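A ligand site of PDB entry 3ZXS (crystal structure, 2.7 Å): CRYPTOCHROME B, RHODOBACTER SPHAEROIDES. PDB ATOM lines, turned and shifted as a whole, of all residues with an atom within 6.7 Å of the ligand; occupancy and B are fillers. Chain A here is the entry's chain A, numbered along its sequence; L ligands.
The backbone NH (N) of Cys 360 sits close to a sulfur (S3) of the ligand, at 3.5 Å. An iron atom (FE2) of the ligand is bound by the side-chain sulfur of Cys 360 (2.2 Å). FE4 of the ligand is bound by SG of Cys 448. The side-chain sulfur (SG) of Cys 464 is bound to an iron atom (FE3) of the ligand (2.3 Å). SG of Cys 451 binds FE1 of the ligand (2.3 Å).
N of Phe 466 lies close to SG of Cys 464, at 3.4 Å. N of Cys 464 is in hydrogen-bond range of O of Ala 454 (3.5 Å). The backbone NH (N) of Ala 359 lies close to the side-chain sulfur (SG) of Cys 451 (3.5 Å). The side-chain sulfur (SG) of Cys 451 sits close to the backbone NH (N) of Tyr 453 (3.4 Å). SG of Cys 451 lies close to O of Arg 357 (3.5 Å). The backbone carbonyl oxygen of Ile 441 sits at hydrogen-bond distance from the side-chain hydroxyl of Ser 445, 2.7 Å away. The backbone NH of Tyr 447 sits at hydrogen-bond distance from the side-chain hydroxyl of Ser 445, 3.0 Å away. The backbone carbonyl oxygen of Val 455 sits at hydrogen-bond distance from the side-chain amide nitrogen of Asn 467, at 2.8 Å.
Merely in contact with the ligand: Met 358 (3.7 Å), Ala 359 (3.7 Å), Ile 441 (3.7 Å), Tyr 447 (3.7 Å), Tyr 453 (3.9 Å) and Val 455 (3.8 Å). Within 4 Å of the ligand: Met 358, Ala 359, Cys 360, Ile 441, Tyr 447, Cys 448, Cys 451, Tyr 453, Val 455 and Cys 464.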
ATOM      1  N   ARG A 357     -10.975  -2.978  -2.765  1.00  0.00           N
ATOM      2  CA  ARG A 357     -10.786  -3.305  -1.373  1.00  0.00           C
ATOM      3  C   ARG A 357     -10.731  -2.076  -0.521  1.00  0.00           C
ATOM      4  O   ARG A 357     -10.696  -2.181   0.692  1.00  0.00           O
ATOM      5  CB  ARG A 357      -9.467  -4.024  -1.198  1.00  0.00           C
ATOM      6  CG  ARG A 357      -9.349  -5.312  -1.944  1.00  0.00           C
ATOM      7  CD  ARG A 357      -9.828  -6.416  -1.098  1.00  0.00           C
ATOM      8  NE  ARG A 357      -9.818  -7.705  -1.771  1.00  0.00           N
ATOM      9  CZ  ARG A 357      -9.857  -8.858  -1.114  1.00  0.00           C
ATOM     10  NH1 ARG A 357      -9.880  -8.895   0.209  1.00  0.00           N
ATOM     11  NH2 ARG A 357      -9.864  -9.984  -1.788  1.00  0.00           N
ATOM     12  N   MET A 358     -10.679  -0.911  -1.141  1.00  0.00           N
ATOM     13  CA  MET A 358     -10.688   0.342  -0.393  1.00  0.00           C
ATOM     14  C   MET A 358     -12.134   0.669   0.034  1.00  0.00           C
ATOM     15  O   MET A 358     -12.993   0.910  -0.783  1.00  0.00           O
ATOM     16  CB  MET A 358     -10.072   1.455  -1.243  1.00  0.00           C
ATOM     17  CG  MET A 358      -8.631   1.142  -1.654  1.00  0.00           C
ATOM     18  SD  MET A 358      -7.901   2.474  -2.597  1.00  0.00           S
ATOM     19  CE  MET A 358      -8.075   1.737  -4.200  1.00  0.00           C
ATOM     20  N   ALA A 359     -12.393   0.589   1.324  1.00  0.00           N
ATOM     21  CA  ALA A 359     -13.763   0.632   1.805  1.00  0.00           C
ATOM     22  C   ALA A 359     -14.411   1.939   1.423  1.00  0.00           C
ATOM     23  O   ALA A 359     -15.482   1.944   0.871  1.00  0.00           O
ATOM     24  CB  ALA A 359     -13.824   0.404   3.287  1.00  0.00           C
ATOM     25  N   CYS A 360     -13.731   3.045   1.688  1.00  0.00           N
ATOM     26  CA  CYS A 360     -14.255   4.380   1.386  1.00  0.00           C
ATOM     27  C   CYS A 360     -14.670   4.532  -0.086  1.00  0.00           C
ATOM     28  O   CYS A 360     -15.770   4.983  -0.373  1.00  0.00           O
ATOM     29  CB  CYS A 360     -13.224   5.469   1.764  1.00  0.00           C
ATOM     30  SG  CYS A 360     -11.457   5.163   1.277  1.00  0.00           S
ATOM     31  N   LEU A 361     -13.784   4.171  -1.000  1.00  0.00           N
ATOM     32  CA  LEU A 361     -14.097   4.290  -2.426  1.00  0.00           C
ATOM     33  C   LEU A 361     -15.242   3.368  -2.849  1.00  0.00           C
ATOM     34  O   LEU A 361     -16.124   3.728  -3.655  1.00  0.00           O
ATOM     35  CB  LEU A 361     -12.839   3.973  -3.260  1.00  0.00           C
ATOM     36  CG  LEU A 361     -11.802   5.071  -3.328  1.00  0.00           C
ATOM     37  CD1 LEU A 361     -10.528   4.602  -3.964  1.00  0.00           C
ATOM     38  CD2 LEU A 361     -12.386   6.289  -4.071  1.00  0.00           C
ATOM     39  N   VAL A 382     -13.170  11.753  -0.947  1.00  0.00           N
ATOM     40  CA  VAL A 382     -12.943  10.357  -1.248  1.00  0.00           C
ATOM     41  C   VAL A 382     -12.640  10.119  -2.712  1.00  0.00           C
ATOM     42  O   VAL A 382     -11.529   9.795  -3.034  1.00  0.00           O
ATOM     43  CB  VAL A 382     -14.078   9.437  -0.780  1.00  0.00           C
ATOM     44  CG1 VAL A 382     -13.735   7.974  -1.167  1.00  0.00           C
ATOM     45  CG2 VAL A 382     -14.274   9.587   0.712  1.00  0.00           C
ATOM     46  N   SER A 437      -4.049  12.120   3.349  1.00  0.00           N
ATOM     47  CA  SER A 437      -3.674  10.756   3.654  1.00  0.00           C
ATOM     48  C   SER A 437      -4.952  10.089   4.141  1.00  0.00           C
ATOM     49  O   SER A 437      -6.025  10.672   4.122  1.00  0.00           O
ATOM     50  CB  SER A 437      -2.618  10.731   4.739  1.00  0.00           C
ATOM     51  OG  SER A 437      -3.180  11.086   5.979  1.00  0.00           O
ATOM     52  N   GLY A 438      -4.853   8.849   4.572  1.00  0.00           N
ATOM     53  CA  GLY A 438      -6.006   8.168   5.114  1.00  0.00           C
ATOM     54  C   GLY A 438      -6.449   8.703   6.449  1.00  0.00           C
ATOM     55  O   GLY A 438      -7.615   8.561   6.800  1.00  0.00           O
ATOM     56  N   ALA A 439      -5.530   9.309   7.213  1.00  0.00           N
ATOM     57  CA  ALA A 439      -5.906   9.850   8.523  1.00  0.00           C
ATOM     58  C   ALA A 439      -7.163  10.694   8.445  1.00  0.00           C
ATOM     59  O   ALA A 439      -7.957  10.629   9.357  1.00  0.00           O
ATOM     60  CB  ALA A 439      -4.782  10.660   9.164  1.00  0.00           C
ATOM     61  N   ILE A 441      -9.804  10.541   6.335  1.00  0.00           N
ATOM     62  CA  ILE A 441     -10.967   9.689   6.140  1.00  0.00           C
ATOM     63  C   ILE A 441     -11.279   8.931   7.430  1.00  0.00           C
ATOM     64  O   ILE A 441     -12.435   8.756   7.807  1.00  0.00           O
ATOM     65  CB  ILE A 441     -10.774   8.742   4.916  1.00  0.00           C
ATOM     66  CG1 ILE A 441     -10.762   9.571   3.613  1.00  0.00           C
ATOM     67  CG2 ILE A 441     -11.876   7.694   4.833  1.00  0.00           C
ATOM     68  CD1 ILE A 441     -10.355   8.795   2.314  1.00  0.00           C
ATOM     69  N   ASP A 442     -10.232   8.520   8.123  1.00  0.00           N
ATOM     70  CA  ASP A 442     -10.398   7.818   9.386  1.00  0.00           C
ATOM     71  C   ASP A 442     -11.043   8.688  10.469  1.00  0.00           C
ATOM     72  O   ASP A 442     -11.861   8.221  11.236  1.00  0.00           O
ATOM     73  CB  ASP A 442      -9.054   7.280   9.883  1.00  0.00           C
ATOM     74  CG  ASP A 442      -9.199   6.322  11.068  1.00  0.00           C
ATOM     75  OD1 ASP A 442     -10.213   5.594  11.161  1.00  0.00           O
ATOM     76  OD2 ASP A 442      -8.287   6.307  11.910  1.00  0.00           O
ATOM     77  N   SER A 445     -14.958   9.479   9.137  1.00  0.00           N
ATOM     78  CA  SER A 445     -15.831   8.367   8.792  1.00  0.00           C
ATOM     79  C   SER A 445     -15.644   7.244   9.784  1.00  0.00           C
ATOM     80  O   SER A 445     -14.779   7.331  10.649  1.00  0.00           O
ATOM     81  CB  SER A 445     -15.512   7.840   7.370  1.00  0.00           C
ATOM     82  OG  SER A 445     -14.410   6.934   7.367  1.00  0.00           O
ATOM     83  N   TYR A 447     -15.261   4.143   8.150  1.00  0.00           N
ATOM     84  CA  TYR A 447     -14.940   3.180   7.096  1.00  0.00           C
ATOM     85  C   TYR A 447     -13.792   2.247   7.439  1.00  0.00           C
ATOM     86  O   TYR A 447     -13.774   1.085   7.051  1.00  0.00           O
ATOM     87  CB  TYR A 447     -14.559   3.890   5.785  1.00  0.00           C
ATOM     88  CG  TYR A 447     -15.677   4.603   5.074  1.00  0.00           C
ATOM     89  CD1 TYR A 447     -16.911   3.984   4.817  1.00  0.00           C
ATOM     90  CD2 TYR A 447     -15.511   5.899   4.620  1.00  0.00           C
ATOM     91  CE1 TYR A 447     -17.939   4.684   4.168  1.00  0.00           C
ATOM     92  CE2 TYR A 447     -16.514   6.583   3.974  1.00  0.00           C
ATOM     93  CZ  TYR A 447     -17.717   5.982   3.738  1.00  0.00           C
ATOM     94  OH  TYR A 447     -18.679   6.709   3.075  1.00  0.00           O
ATOM     95  N   CYS A 448     -12.822   2.758   8.175  1.00  0.00           N
ATOM     96  CA  CYS A 448     -11.499   2.167   8.159  1.00  0.00           C
ATOM     97  C   CYS A 448     -11.406   0.854   8.934  1.00  0.00           C
ATOM     98  O   CYS A 448     -10.584  -0.038   8.581  1.00  0.00           O
ATOM     99  CB  CYS A 448     -10.452   3.203   8.607  1.00  0.00           C
ATOM    100  SG  CYS A 448     -10.226   4.574   7.404  1.00  0.00           S
ATOM    101  N   ARG A 449     -12.244   0.711   9.959  1.00  0.00           N
ATOM    102  CA  ARG A 449     -12.296  -0.533  10.720  1.00  0.00           C
ATOM    103  C   ARG A 449     -12.810  -1.713   9.880  1.00  0.00           C
ATOM    104  O   ARG A 449     -12.380  -2.827  10.073  1.00  0.00           O
ATOM    105  CB  ARG A 449     -13.108  -0.395  12.007  1.00  0.00           C
ATOM    106  CG  ARG A 449     -12.718  -1.491  13.101  1.00  0.00           C
ATOM    107  CD  ARG A 449     -13.662  -1.577  14.340  1.00  0.00           C
ATOM    108  NE  ARG A 449     -15.090  -1.765  13.997  1.00  0.00           N
ATOM    109  CZ  ARG A 449     -16.088  -1.841  14.877  1.00  0.00           C
ATOM    110  NH1 ARG A 449     -15.854  -1.754  16.188  1.00  0.00           N
ATOM    111  NH2 ARG A 449     -17.343  -1.984  14.450  1.00  0.00           N
ATOM    112  N   GLY A 450     -13.713  -1.440   8.952  1.00  0.00           N
ATOM    113  CA  GLY A 450     -14.182  -2.427   7.985  1.00  0.00           C
ATOM    114  C   GLY A 450     -13.336  -2.670   6.746  1.00  0.00           C
ATOM    115  O   GLY A 450     -13.676  -3.510   5.922  1.00  0.00           O
ATOM    116  N   CYS A 451     -12.223  -1.962   6.626  1.00  0.00           N
ATOM    117  CA  CYS A 451     -11.412  -2.003   5.426  1.00  0.00           C
ATOM    118  C   CYS A 451     -10.225  -2.962   5.572  1.00  0.00           C
ATOM    119  O   CYS A 451      -9.631  -3.031   6.626  1.00  0.00           O
ATOM    120  CB  CYS A 451     -10.919  -0.599   5.128  1.00  0.00           C
ATOM    121  SG  CYS A 451      -9.959  -0.419   3.635  1.00  0.00           S
ATOM    122  N   ALA A 452      -9.874  -3.701   4.536  1.00  0.00           N
ATOM    123  CA  ALA A 452      -8.734  -4.621   4.601  1.00  0.00           C
ATOM    124  C   ALA A 452      -7.429  -3.862   4.743  1.00  0.00           C
ATOM    125  O   ALA A 452      -6.449  -4.422   5.273  1.00  0.00           O
ATOM    126  CB  ALA A 452      -8.694  -5.526   3.379  1.00  0.00           C
ATOM    127  N   TYR A 453      -7.385  -2.601   4.314  1.00  0.00           N
ATOM    128  CA  TYR A 453      -6.189  -1.796   4.493  1.00  0.00           C
ATOM    129  C   TYR A 453      -6.058  -1.339   5.950  1.00  0.00           C
ATOM    130  O   TYR A 453      -7.036  -1.327   6.681  1.00  0.00           O
ATOM    131  CB  TYR A 453      -6.141  -0.619   3.506  1.00  0.00           C
ATOM    132  CG  TYR A 453      -5.951  -1.055   2.058  1.00  0.00           C
ATOM    133  CD1 TYR A 453      -4.706  -1.453   1.572  1.00  0.00           C
ATOM    134  CD2 TYR A 453      -7.017  -1.086   1.184  1.00  0.00           C
ATOM    135  CE1 TYR A 453      -4.550  -1.851   0.257  1.00  0.00           C
ATOM    136  CE2 TYR A 453      -6.869  -1.500  -0.144  1.00  0.00           C
ATOM    137  CZ  TYR A 453      -5.649  -1.872  -0.594  1.00  0.00           C
ATOM    138  OH  TYR A 453      -5.550  -2.266  -1.903  1.00  0.00           O
ATOM    139  N   ALA A 454      -4.837  -1.011   6.345  1.00  0.00           N
ATOM    140  CA  ALA A 454      -4.526  -0.503   7.692  1.00  0.00           C
ATOM    141  C   ALA A 454      -4.210   0.986   7.637  1.00  0.00           C
ATOM    142  O   ALA A 454      -3.141   1.382   7.183  1.00  0.00           O
ATOM    143  CB  ALA A 454      -3.328  -1.266   8.303  1.00  0.00           C
ATOM    144  N   VAL A 455      -5.128   1.811   8.105  1.00  0.00           N
ATOM    145  CA  VAL A 455      -4.990   3.231   7.932  1.00  0.00           C
ATOM    146  C   VAL A 455      -3.820   3.787   8.705  1.00  0.00           C
ATOM    147  O   VAL A 455      -3.274   4.794   8.317  1.00  0.00           O
ATOM    148  CB  VAL A 455      -6.293   3.970   8.322  1.00  0.00           C
ATOM    149  CG1 VAL A 455      -6.465   4.053   9.844  1.00  0.00           C
ATOM    150  CG2 VAL A 455      -6.283   5.330   7.678  1.00  0.00           C
ATOM    151  N   LYS A 456      -3.403   3.133   9.787  1.00  0.00           N
ATOM    152  CA  LYS A 456      -2.279   3.612  10.629  1.00  0.00           C
ATOM    153  C   LYS A 456      -0.945   3.111  10.080  1.00  0.00           C
ATOM    154  O   LYS A 456       0.071   3.498  10.578  1.00  0.00           O
ATOM    155  CB  LYS A 456      -2.429   3.207  12.124  1.00  0.00           C
ATOM    156  CG  LYS A 456      -3.789   3.572  12.824  1.00  0.00           C
ATOM    157  CD  LYS A 456      -3.818   4.904  13.636  1.00  0.00           C
ATOM    158  N   ARG A 462      -0.199  -3.766   3.832  1.00  0.00           N
ATOM    159  CA  ARG A 462      -1.468  -3.253   4.320  1.00  0.00           C
ATOM    160  C   ARG A 462      -1.628  -1.716   4.302  1.00  0.00           C
ATOM    161  O   ARG A 462      -2.706  -1.191   4.608  1.00  0.00           O
ATOM    162  CB  ARG A 462      -1.702  -3.733   5.752  1.00  0.00           C
ATOM    163  CG  ARG A 462      -2.711  -4.837   5.910  1.00  0.00           C
ATOM    164  CD  ARG A 462      -2.082  -6.202   6.041  1.00  0.00           C
ATOM    165  NE  ARG A 462      -1.089  -6.219   7.109  1.00  0.00           N
ATOM    166  CZ  ARG A 462      -0.231  -7.231   7.320  1.00  0.00           C
ATOM    167  NH1 ARG A 462      -0.269  -8.318   6.541  1.00  0.00           N
ATOM    168  NH2 ARG A 462       0.653  -7.139   8.304  1.00  0.00           N
ATOM    169  N   ALA A 463      -0.552  -1.012   3.952  1.00  0.00           N
ATOM    170  CA  ALA A 463      -0.568   0.472   3.950  1.00  0.00           C
ATOM    171  C   ALA A 463      -1.749   1.077   3.145  1.00  0.00           C
ATOM    172  O   ALA A 463      -1.917   0.807   1.973  1.00  0.00           O
ATOM    173  CB  ALA A 463       0.740   0.989   3.433  1.00  0.00           C
ATOM    174  N   CYS A 464      -2.584   1.873   3.797  1.00  0.00           N
ATOM    175  CA  CYS A 464      -3.726   2.543   3.145  1.00  0.00           C
ATOM    176  C   CYS A 464      -3.193   3.243   1.952  1.00  0.00           C
ATOM    177  O   CYS A 464      -2.198   3.953   2.053  1.00  0.00           O
ATOM    178  CB  CYS A 464      -4.382   3.583   4.065  1.00  0.00           C
ATOM    179  SG  CYS A 464      -5.584   4.716   3.290  1.00  0.00           S
ATOM    180  N   PRO A 465      -3.847   3.076   0.802  1.00  0.00           N
ATOM    181  CA  PRO A 465      -3.272   3.713  -0.377  1.00  0.00           C
ATOM    182  C   PRO A 465      -3.240   5.242  -0.363  1.00  0.00           C
ATOM    183  O   PRO A 465      -2.385   5.813  -1.031  1.00  0.00           O
ATOM    184  CB  PRO A 465      -4.092   3.149  -1.516  1.00  0.00           C
ATOM    185  CG  PRO A 465      -4.560   1.847  -0.978  1.00  0.00           C
ATOM    186  CD  PRO A 465      -4.850   2.076   0.443  1.00  0.00           C
ATOM    187  N   PHE A 466      -4.099   5.896   0.409  1.00  0.00           N
ATOM    188  CA  PHE A 466      -4.011   7.327   0.509  1.00  0.00           C
ATOM    189  C   PHE A 466      -2.739   7.693   1.250  1.00  0.00           C
ATOM    190  O   PHE A 466      -2.143   8.758   0.994  1.00  0.00           O
ATOM    191  CB  PHE A 466      -5.228   7.939   1.198  1.00  0.00           C
ATOM    192  CG  PHE A 466      -6.513   7.882   0.405  1.00  0.00           C
ATOM    193  CD1 PHE A 466      -7.317   6.765   0.425  1.00  0.00           C
ATOM    194  CD2 PHE A 466      -6.956   8.970  -0.315  1.00  0.00           C
ATOM    195  CE1 PHE A 466      -8.531   6.727  -0.298  1.00  0.00           C
ATOM    196  CE2 PHE A 466      -8.184   8.941  -1.064  1.00  0.00           C
ATOM    197  CZ  PHE A 466      -8.958   7.837  -1.032  1.00  0.00           C
ATOM    198  N   ASN A 467      -2.273   6.823   2.151  1.00  0.00           N
ATOM    199  CA  ASN A 467      -1.043   7.135   2.869  1.00  0.00           C
ATOM    200  C   ASN A 467       0.147   7.149   1.889  1.00  0.00           C
ATOM    201  O   ASN A 467       1.021   7.991   1.998  1.00  0.00           O
ATOM    202  CB  ASN A 467      -0.763   6.161   4.009  1.00  0.00           C
ATOM    203  CG  ASN A 467      -1.798   6.225   5.140  1.00  0.00           C
ATOM    204  OD1 ASN A 467      -2.573   7.177   5.286  1.00  0.00           O
ATOM    205  ND2 ASN A 467      -1.806   5.186   5.972  1.00  0.00           N
HETATM  206 FE1  LIG L   1      -9.401   1.762   3.713  1.00  0.00          FE
HETATM  207 FE2  LIG L   1     -10.184   4.220   2.782  1.00  0.00          FE
HETATM  208 FE3  LIG L   1      -7.632   3.837   3.605  1.00  0.00          FE
HETATM  209 FE4  LIG L   1      -9.623   3.925   5.379  1.00  0.00          FE
HETATM  210  S1  LIG L   1      -8.929   5.652   4.049  1.00  0.00           S
HETATM  211  S2  LIG L   1      -7.914   2.372   5.305  1.00  0.00           S
HETATM  212  S3  LIG L   1     -11.344   2.926   4.246  1.00  0.00           S
HETATM  213  S4  LIG L   1      -8.641   2.792   1.867  1.00  0.00           S
